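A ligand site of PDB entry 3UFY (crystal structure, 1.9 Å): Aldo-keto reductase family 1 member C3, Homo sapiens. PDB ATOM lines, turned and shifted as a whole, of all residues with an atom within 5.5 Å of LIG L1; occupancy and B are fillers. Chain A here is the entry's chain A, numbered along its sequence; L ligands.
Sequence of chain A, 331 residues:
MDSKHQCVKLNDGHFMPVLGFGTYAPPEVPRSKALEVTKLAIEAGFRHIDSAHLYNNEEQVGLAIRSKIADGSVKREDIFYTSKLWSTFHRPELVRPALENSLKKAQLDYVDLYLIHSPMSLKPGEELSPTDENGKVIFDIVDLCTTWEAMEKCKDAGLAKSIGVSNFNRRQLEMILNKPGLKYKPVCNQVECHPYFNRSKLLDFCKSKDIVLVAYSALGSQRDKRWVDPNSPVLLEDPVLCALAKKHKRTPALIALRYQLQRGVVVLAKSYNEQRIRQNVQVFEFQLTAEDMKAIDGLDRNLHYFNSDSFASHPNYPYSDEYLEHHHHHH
The backbone NH of Met 120 is in hydrogen-bond range of the side-chain hydroxyl of Ser 118, at 3.1 Å.
The side-chain hydroxyl (OH) of Tyr 55 lies within hydrogen-bond range of the side-chain amino group (NZ) of Lys 84, 3.1 Å away.
ND2 of Asn 167 sits at hydrogen-bond distance from O of His 117 (3.0 Å).
The side-chain hydroxyl (OH) of Tyr 216 lies within hydrogen-bond range of the side-chain amide oxygen (OD1) of Asn 167, at 2.5 Å.
ND2 of Asn 167 is in hydrogen-bond range of O14 of LG2 L2 (2.8 Å).
O2 of LIG L1 sits at hydrogen-bond distance from NE2 of His 117 (2.8 Å).
The side-chain hydroxyl (OH) of Tyr 55 sits at hydrogen-bond distance from an oxygen (O2) of LIG L1 (2.5 Å).
The backbone NH (N) of Tyr 24 sits at hydrogen-bond distance from an oxygen (O12) of LG2 L2.
A ring nitrogen (NE2) of His 117 sits at hydrogen-bond distance from an oxygen (O14) of LG2 L2 (3.4 Å).
Merely in contact with LIG L1: Leu 54 (3.7 Å), Ser 118 (3.6 Å), Met 120 (3.2 Å), Asn 167 (3.4 Å), Tyr 216 (3.5 Å), Trp 227 (3.7 Å), Phe 306 (3.4 Å), Phe 311 (3.6 Å), Pro 318 (3.7 Å) and Tyr 319 (3.6 Å).
Hydrophobic or aromatic side chains within 4 Å of LIG L1: Leu 54, Tyr 55, His 117, Met 120, Trp 227, Phe 306, Phe 311, Pro 318 and Tyr 319.
Of the 16 residues printed, 12 come within 4 Å of LIG L1.
Along chain A the residues within 4 Å of LIG L1 span positions 54 to 319.
The nearest printed residue that does not touch LIG L1 is Tyr 24 (4.2 Å).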
ATOM      1  N   TYR A  24       9.193   7.383 -20.533  1.00  0.00           N
ATOM      2  CA  TYR A  24      10.305   8.055 -19.870  1.00  0.00           C
ATOM      3  C   TYR A  24       9.787   9.283 -19.094  1.00  0.00           C
ATOM      4  O   TYR A  24       8.990  10.026 -19.637  1.00  0.00           O
ATOM      5  CB  TYR A  24      11.414   8.528 -20.859  1.00  0.00           C
ATOM      6  CG  TYR A  24      12.493   9.222 -20.071  1.00  0.00           C
ATOM      7  CD1 TYR A  24      13.445   8.438 -19.349  1.00  0.00           C
ATOM      8  CD2 TYR A  24      12.568  10.618 -19.969  1.00  0.00           C
ATOM      9  CE1 TYR A  24      14.420   9.013 -18.557  1.00  0.00           C
ATOM     10  CE2 TYR A  24      13.605  11.217 -19.179  1.00  0.00           C
ATOM     11  CZ  TYR A  24      14.491  10.414 -18.479  1.00  0.00           C
ATOM     12  OH  TYR A  24      15.457  10.990 -17.702  1.00  0.00           O
ATOM     13  N   LEU A  54      17.594   2.075 -19.036  1.00  0.00           N
ATOM     14  CA  LEU A  54      17.953   3.458 -18.682  1.00  0.00           C
ATOM     15  C   LEU A  54      16.856   4.230 -17.914  1.00  0.00           C
ATOM     16  O   LEU A  54      17.189   5.116 -17.118  1.00  0.00           O
ATOM     17  CB  LEU A  54      18.287   4.292 -19.912  1.00  0.00           C
ATOM     18  CG  LEU A  54      18.987   5.698 -19.751  1.00  0.00           C
ATOM     19  CD1 LEU A  54      20.375   5.649 -19.100  1.00  0.00           C
ATOM     20  CD2 LEU A  54      19.048   6.416 -21.118  1.00  0.00           C
ATOM     21  N   TYR A  55      15.570   3.901 -18.184  1.00  0.00           N
ATOM     22  CA  TYR A  55      14.474   4.771 -17.659  1.00  0.00           C
ATOM     23  C   TYR A  55      14.230   4.595 -16.187  1.00  0.00           C
ATOM     24  O   TYR A  55      13.481   5.421 -15.580  1.00  0.00           O
ATOM     25  CB  TYR A  55      13.175   4.537 -18.435  1.00  0.00           C
ATOM     26  CG  TYR A  55      13.331   4.758 -19.944  1.00  0.00           C
ATOM     27  CD1 TYR A  55      14.486   5.445 -20.456  1.00  0.00           C
ATOM     28  CD2 TYR A  55      12.321   4.400 -20.829  1.00  0.00           C
ATOM     29  CE1 TYR A  55      14.626   5.634 -21.891  1.00  0.00           C
ATOM     30  CE2 TYR A  55      12.416   4.606 -22.234  1.00  0.00           C
ATOM     31  CZ  TYR A  55      13.565   5.244 -22.727  1.00  0.00           C
ATOM     32  OH  TYR A  55      13.739   5.430 -24.081  1.00  0.00           O
ATOM     33  N   LYS A  84      15.180  -2.035 -23.697  1.00  0.00           N
ATOM     34  CA  LYS A  84      16.338  -1.633 -24.505  1.00  0.00           C
ATOM     35  C   LYS A  84      17.577  -1.929 -23.712  1.00  0.00           C
ATOM     36  O   LYS A  84      17.660  -1.679 -22.493  1.00  0.00           O
ATOM     37  CB  LYS A  84      16.312  -0.163 -24.898  1.00  0.00           C
ATOM     38  CG  LYS A  84      14.951   0.290 -25.545  1.00  0.00           C
ATOM     39  CD  LYS A  84      15.148   1.728 -26.052  1.00  0.00           C
ATOM     40  CE  LYS A  84      13.730   2.309 -26.467  1.00  0.00           C
ATOM     41  NZ  LYS A  84      12.958   2.733 -25.303  1.00  0.00           N
ATOM     42  N   TRP A  86      21.149  -1.065 -22.557  1.00  0.00           N
ATOM     43  CA  TRP A  86      21.881   0.181 -22.446  1.00  0.00           C
ATOM     44  C   TRP A  86      23.348  -0.002 -22.925  1.00  0.00           C
ATOM     45  O   TRP A  86      23.847  -1.133 -23.013  1.00  0.00           O
ATOM     46  CB  TRP A  86      21.764   0.757 -20.961  1.00  0.00           C
ATOM     47  CG  TRP A  86      22.491   2.107 -20.904  1.00  0.00           C
ATOM     48  CD1 TRP A  86      23.561   2.439 -20.100  1.00  0.00           C
ATOM     49  CD2 TRP A  86      22.273   3.206 -21.788  1.00  0.00           C
ATOM     50  NE1 TRP A  86      24.013   3.709 -20.406  1.00  0.00           N
ATOM     51  CE2 TRP A  86      23.239   4.202 -21.451  1.00  0.00           C
ATOM     52  CE3 TRP A  86      21.345   3.460 -22.838  1.00  0.00           C
ATOM     53  CZ2 TRP A  86      23.303   5.437 -22.101  1.00  0.00           C
ATOM     54  CZ3 TRP A  86      21.393   4.732 -23.507  1.00  0.00           C
ATOM     55  CH2 TRP A  86      22.385   5.689 -23.136  1.00  0.00           C
ATOM     56  N   HIS A 117      19.932   0.106 -27.555  1.00  0.00           N
ATOM     57  CA  HIS A 117      19.368   1.430 -27.311  1.00  0.00           C
ATOM     58  C   HIS A 117      20.113   2.469 -28.188  1.00  0.00           C
ATOM     59  O   HIS A 117      19.528   3.511 -28.574  1.00  0.00           O
ATOM     60  CB  HIS A 117      19.562   1.801 -25.801  1.00  0.00           C
ATOM     61  CG  HIS A 117      18.620   2.863 -25.283  1.00  0.00           C
ATOM     62  ND1 HIS A 117      18.158   2.890 -23.976  1.00  0.00           N
ATOM     63  CD2 HIS A 117      18.162   3.991 -25.861  1.00  0.00           C
ATOM     64  CE1 HIS A 117      17.419   3.967 -23.793  1.00  0.00           C
ATOM     65  NE2 HIS A 117      17.392   4.655 -24.924  1.00  0.00           N
ATOM     66  N   SER A 118      21.403   2.223 -28.402  1.00  0.00           N
ATOM     67  CA  SER A 118      22.221   3.252 -29.026  1.00  0.00           C
ATOM     68  C   SER A 118      23.468   2.594 -29.588  1.00  0.00           C
ATOM     69  O   SER A 118      23.929   1.622 -29.024  1.00  0.00           O
ATOM     70  CB  SER A 118      22.600   4.302 -27.954  1.00  0.00           C
ATOM     71  OG  SER A 118      23.670   5.143 -28.385  1.00  0.00           O
ATOM     72  N   MET A 120      26.273   3.978 -29.534  1.00  0.00           N
ATOM     73  CA  MET A 120      27.447   4.635 -28.972  1.00  0.00           C
ATOM     74  C   MET A 120      27.890   3.956 -27.680  1.00  0.00           C
ATOM     75  O   MET A 120      27.359   4.228 -26.563  1.00  0.00           O
ATOM     76  CB  MET A 120      27.136   6.106 -28.692  1.00  0.00           C
ATOM     77  CG  MET A 120      26.982   6.947 -29.996  1.00  0.00           C
ATOM     78  SD  MET A 120      26.418   8.620 -29.595  1.00  0.00           S
ATOM     79  CE  MET A 120      24.669   8.339 -29.234  1.00  0.00           C
ATOM     80  N   ASN A 167      18.501   4.480 -32.682  1.00  0.00           N
ATOM     81  CA  ASN A 167      19.520   5.508 -32.918  1.00  0.00           C
ATOM     82  C   ASN A 167      20.594   5.112 -33.878  1.00  0.00           C
ATOM     83  O   ASN A 167      21.698   5.711 -33.864  1.00  0.00           O
ATOM     84  CB  ASN A 167      20.097   6.038 -31.560  1.00  0.00           C
ATOM     85  CG  ASN A 167      19.026   6.741 -30.754  1.00  0.00           C
ATOM     86  OD1 ASN A 167      18.467   7.754 -31.192  1.00  0.00           O
ATOM     87  ND2 ASN A 167      18.740   6.203 -29.550  1.00  0.00           N
ATOM     88  N   TYR A 216      10.490   8.317 -31.995  1.00  0.00           N
ATOM     89  CA  TYR A 216      10.441   8.913 -30.632  1.00  0.00           C
ATOM     90  C   TYR A 216      10.603  10.406 -30.737  1.00  0.00           C
ATOM     91  O   TYR A 216      11.039  10.944 -31.754  1.00  0.00           O
ATOM     92  CB  TYR A 216      11.486   8.304 -29.691  1.00  0.00           C
ATOM     93  CG  TYR A 216      12.963   8.672 -29.923  1.00  0.00           C
ATOM     94  CD1 TYR A 216      13.427   9.944 -29.630  1.00  0.00           C
ATOM     95  CD2 TYR A 216      13.900   7.706 -30.339  1.00  0.00           C
ATOM     96  CE1 TYR A 216      14.797  10.282 -29.792  1.00  0.00           C
ATOM     97  CE2 TYR A 216      15.264   8.004 -30.447  1.00  0.00           C
ATOM     98  CZ  TYR A 216      15.694   9.300 -30.152  1.00  0.00           C
ATOM     99  OH  TYR A 216      17.047   9.642 -30.276  1.00  0.00           O
ATOM    100  N   TRP A 227      19.957  17.678 -22.488  1.00  0.00           N
ATOM    101  CA  TRP A 227      20.303  17.409 -23.919  1.00  0.00           C
ATOM    102  C   TRP A 227      19.684  18.356 -24.925  1.00  0.00           C
ATOM    103  O   TRP A 227      20.127  18.361 -26.076  1.00  0.00           O
ATOM    104  CB  TRP A 227      19.848  15.995 -24.333  1.00  0.00           C
ATOM    105  CG  TRP A 227      20.213  14.943 -23.318  1.00  0.00           C
ATOM    106  CD1 TRP A 227      21.483  14.444 -23.068  1.00  0.00           C
ATOM    107  CD2 TRP A 227      19.333  14.284 -22.400  1.00  0.00           C
ATOM    108  NE1 TRP A 227      21.446  13.542 -22.007  1.00  0.00           N
ATOM    109  CE2 TRP A 227      20.128  13.379 -21.621  1.00  0.00           C
ATOM    110  CE3 TRP A 227      17.929  14.304 -22.194  1.00  0.00           C
ATOM    111  CZ2 TRP A 227      19.585  12.543 -20.616  1.00  0.00           C
ATOM    112  CZ3 TRP A 227      17.373  13.459 -21.230  1.00  0.00           C
ATOM    113  CH2 TRP A 227      18.220  12.587 -20.431  1.00  0.00           C
ATOM    114  N   PHE A 306      17.759  16.356 -29.469  1.00  0.00           N
ATOM    115  CA  PHE A 306      18.885  15.846 -28.635  1.00  0.00           C
ATOM    116  C   PHE A 306      20.189  16.292 -29.256  1.00  0.00           C
ATOM    117  O   PHE A 306      20.598  15.785 -30.308  1.00  0.00           O
ATOM    118  CB  PHE A 306      18.812  14.313 -28.480  1.00  0.00           C
ATOM    119  CG  PHE A 306      17.639  13.882 -27.652  1.00  0.00           C
ATOM    120  CD1 PHE A 306      17.762  13.736 -26.272  1.00  0.00           C
ATOM    121  CD2 PHE A 306      16.380  13.745 -28.218  1.00  0.00           C
ATOM    122  CE1 PHE A 306      16.659  13.410 -25.477  1.00  0.00           C
ATOM    123  CE2 PHE A 306      15.273  13.382 -27.423  1.00  0.00           C
ATOM    124  CZ  PHE A 306      15.436  13.205 -26.045  1.00  0.00           C
ATOM    125  N   PHE A 311      26.696  13.216 -26.802  1.00  0.00           N
ATOM    126  CA  PHE A 311      26.499  12.296 -27.952  1.00  0.00           C
ATOM    127  C   PHE A 311      27.486  12.689 -29.071  1.00  0.00           C
ATOM    128  O   PHE A 311      28.129  11.824 -29.711  1.00  0.00           O
ATOM    129  CB  PHE A 311      25.094  12.459 -28.492  1.00  0.00           C
ATOM    130  CG  PHE A 311      24.008  12.136 -27.510  1.00  0.00           C
ATOM    131  CD1 PHE A 311      24.009  10.929 -26.803  1.00  0.00           C
ATOM    132  CD2 PHE A 311      22.931  13.039 -27.327  1.00  0.00           C
ATOM    133  CE1 PHE A 311      22.943  10.629 -25.885  1.00  0.00           C
ATOM    134  CE2 PHE A 311      21.902  12.735 -26.405  1.00  0.00           C
ATOM    135  CZ  PHE A 311      21.918  11.545 -25.698  1.00  0.00           C
ATOM    136  N   TYR A 317      28.728   8.484 -33.167  1.00  0.00           N
ATOM    137  CA  TYR A 317      27.589   9.395 -33.109  1.00  0.00           C
ATOM    138  C   TYR A 317      26.787   9.200 -34.377  1.00  0.00           C
ATOM    139  O   TYR A 317      27.338   9.345 -35.456  1.00  0.00           O
ATOM    140  CB  TYR A 317      28.124  10.827 -33.136  1.00  0.00           C
ATOM    141  CG  TYR A 317      27.095  11.938 -33.091  1.00  0.00           C
ATOM    142  CD1 TYR A 317      26.065  11.926 -32.172  1.00  0.00           C
ATOM    143  CD2 TYR A 317      27.249  13.065 -33.909  1.00  0.00           C
ATOM    144  CE1 TYR A 317      25.155  13.023 -32.113  1.00  0.00           C
ATOM    145  CE2 TYR A 317      26.413  14.158 -33.841  1.00  0.00           C
ATOM    146  CZ  TYR A 317      25.349  14.086 -32.941  1.00  0.00           C
ATOM    147  OH  TYR A 317      24.518  15.145 -32.847  1.00  0.00           O
ATOM    148  N   PRO A 318      25.497   8.916 -34.244  1.00  0.00           N
ATOM    149  CA  PRO A 318      24.743   8.621 -35.450  1.00  0.00           C
ATOM    150  C   PRO A 318      24.487   9.800 -36.398  1.00  0.00           C
ATOM    151  O   PRO A 318      24.325   9.612 -37.624  1.00  0.00           O
ATOM    152  CB  PRO A 318      23.446   8.013 -34.890  1.00  0.00           C
ATOM    153  CG  PRO A 318      23.278   8.655 -33.599  1.00  0.00           C
ATOM    154  CD  PRO A 318      24.708   8.620 -33.027  1.00  0.00           C
ATOM    155  N   TYR A 319      24.524  11.017 -35.889  1.00  0.00           N
ATOM    156  CA  TYR A 319      24.239  12.134 -36.764  1.00  0.00           C
ATOM    157  C   TYR A 319      25.492  12.670 -37.474  1.00  0.00           C
ATOM    158  O   TYR A 319      25.435  13.734 -38.052  1.00  0.00           O
ATOM    159  CB  TYR A 319      23.546  13.254 -35.979  1.00  0.00           C
ATOM    160  CG  TYR A 319      22.282  12.763 -35.285  1.00  0.00           C
ATOM    161  CD1 TYR A 319      21.438  11.854 -35.905  1.00  0.00           C
ATOM    162  CD2 TYR A 319      21.928  13.241 -34.038  1.00  0.00           C
ATOM    163  CE1 TYR A 319      20.202  11.436 -35.302  1.00  0.00           C
ATOM    164  CE2 TYR A 319      20.747  12.824 -33.435  1.00  0.00           C
ATOM    165  CZ  TYR A 319      19.891  11.919 -34.048  1.00  0.00           C
ATOM    166  OH  TYR A 319      18.729  11.485 -33.418  1.00  0.00           O
HETATM  167  C1  LIG L   1      20.991   8.967 -28.887  1.00  0.00           C
HETATM  168  O1  LIG L   1      21.652   9.144 -30.045  1.00  0.00           O
HETATM  169  C2  LIG L   1      21.335   7.878 -28.113  1.00  0.00           C
HETATM  170  C3  LIG L   1      20.675   7.582 -26.941  1.00  0.00           C
HETATM  171  C4  LIG L   1      19.671   8.411 -26.511  1.00  0.00           C
HETATM  172  C5  LIG L   1      19.331   9.544 -27.248  1.00  0.00           C
HETATM  173  C6  LIG L   1      19.979   9.802 -28.458  1.00  0.00           C
HETATM  174  C7  LIG L   1      19.030   8.117 -25.296  1.00  0.00           C
HETATM  175  C8  LIG L   1      18.016   8.925 -24.841  1.00  0.00           C
HETATM  176  C9  LIG L   1      17.329   8.561 -23.564  1.00  0.00           C
HETATM  177  C10 LIG L   1      17.311   9.677 -22.501  1.00  0.00           C
HETATM  178  C11 LIG L   1      18.299  10.398 -26.779  1.00  0.00           C
HETATM  179  C12 LIG L   1      17.613  10.089 -25.598  1.00  0.00           C
HETATM  180  C13 LIG L   1      21.432  10.324 -30.898  1.00  0.00           C
HETATM  181  O2  LIG L   1      15.782   6.905 -24.366  1.00  0.00           O
HETATM  182  O3  LIG L   1      14.880   8.733 -23.488  1.00  0.00           O
HETATM  183  C14 LIG L   1      15.929   8.069 -23.834  1.00  0.00           C
HETATM  184  P1  LG2 L   2       7.137  13.014 -26.768  1.00  0.00           P
HETATM  185  O1  LG2 L   2       6.350  11.798 -27.073  1.00  0.00           O
HETATM  186  O2  LG2 L   2       7.894  13.774 -27.891  1.00  0.00           O
HETATM  187  O3  LG2 L   2       6.339  14.099 -25.881  1.00  0.00           O
HETATM  188  C1  LG2 L   2       6.835  15.424 -25.650  1.00  0.00           C
HETATM  189  C2  LG2 L   2       5.872  16.068 -24.645  1.00  0.00           C
HETATM  190  O4  LG2 L   2       4.552  16.082 -25.321  1.00  0.00           O
HETATM  191  C3  LG2 L   2       5.587  15.198 -23.415  1.00  0.00           C
HETATM  192  O5  LG2 L   2       6.437  15.507 -22.287  1.00  0.00           O
HETATM  193  C4  LG2 L   2       4.071  15.455 -23.095  1.00  0.00           C
HETATM  194  O6  LG2 L   2       3.839  16.268 -21.944  1.00  0.00           O
HETATM  195  C5  LG2 L   2       3.574  16.236 -24.282  1.00  0.00           C
HETATM  196  N1  LG2 L   2       2.282  15.767 -24.847  1.00  0.00           N
HETATM  197  C6  LG2 L   2       1.873  14.487 -24.984  1.00  0.00           C
HETATM  198  N2  LG2 L   2       0.652  14.483 -25.566  1.00  0.00           N
HETATM  199  C7  LG2 L   2       0.290  15.734 -25.768  1.00  0.00           C
HETATM  200  C8  LG2 L   2      -0.882  16.276 -26.312  1.00  0.00           C
HETATM  201  N3  LG2 L   2      -1.928  15.470 -26.757  1.00  0.00           N
HETATM  202  N4  LG2 L   2      -0.955  17.620 -26.355  1.00  0.00           N
HETATM  203  C9  LG2 L   2       0.040  18.446 -25.904  1.00  0.00           C
HETATM  204  N5  LG2 L   2       1.206  17.968 -25.391  1.00  0.00           N
HETATM  205  C10 LG2 L   2       1.326  16.579 -25.306  1.00  0.00           C
HETATM  206  O7  LG2 L   2       8.235  12.633 -25.644  1.00  0.00           O
HETATM  207  P2  LG2 L   2       9.583  11.747 -25.516  1.00  0.00           P
HETATM  208  O8  LG2 L   2       9.563  11.274 -24.103  1.00  0.00           O
HETATM  209  O9  LG2 L   2      10.720  12.630 -25.963  1.00  0.00           O
HETATM  210  O10 LG2 L   2       9.409  10.560 -26.591  1.00  0.00           O
HETATM  211  C11 LG2 L   2       8.359   9.542 -26.354  1.00  0.00           C
HETATM  212  C12 LG2 L   2       9.044   8.243 -25.846  1.00  0.00           C
HETATM  213  O11 LG2 L   2      10.036   7.753 -26.799  1.00  0.00           O
HETATM  214  C13 LG2 L   2       9.849   8.376 -24.593  1.00  0.00           C
HETATM  215  O12 LG2 L   2       9.014   8.433 -23.427  1.00  0.00           O
HETATM  216  C14 LG2 L   2      10.645   7.043 -24.572  1.00  0.00           C
HETATM  217  O13 LG2 L   2       9.667   5.961 -24.365  1.00  0.00           O
HETATM  218  C15 LG2 L   2      11.025   6.967 -26.072  1.00  0.00           C
HETATM  219  N6  LG2 L   2      12.367   7.622 -26.389  1.00  0.00           N
HETATM  220  C16 LG2 L   2      13.349   6.772 -26.801  1.00  0.00           C
HETATM  221  C17 LG2 L   2      14.621   7.274 -27.097  1.00  0.00           C
HETATM  222  C18 LG2 L   2      15.698   6.344 -27.589  1.00  0.00           C
HETATM  223  O14 LG2 L   2      16.875   6.727 -27.533  1.00  0.00           O
HETATM  224  N7  LG2 L   2      15.249   5.193 -28.158  1.00  0.00           N
HETATM  225  C19 LG2 L   2      14.907   8.593 -26.847  1.00  0.00           C
HETATM  226  C20 LG2 L   2      13.901   9.482 -26.424  1.00  0.00           C
HETATM  227  C21 LG2 L   2      12.600   9.039 -26.192  1.00  0.00           C
HETATM  228  P3  LG2 L   2       2.854  15.686 -20.717  1.00  0.00           P
HETATM  229  O15 LG2 L   2       3.561  14.485 -20.096  1.00  0.00           O
HETATM  230  O16 LG2 L   2       2.724  16.878 -19.828  1.00  0.00           O
HETATM  231  O17 LG2 L   2       1.455  15.393 -21.450  1.00  0.00           O
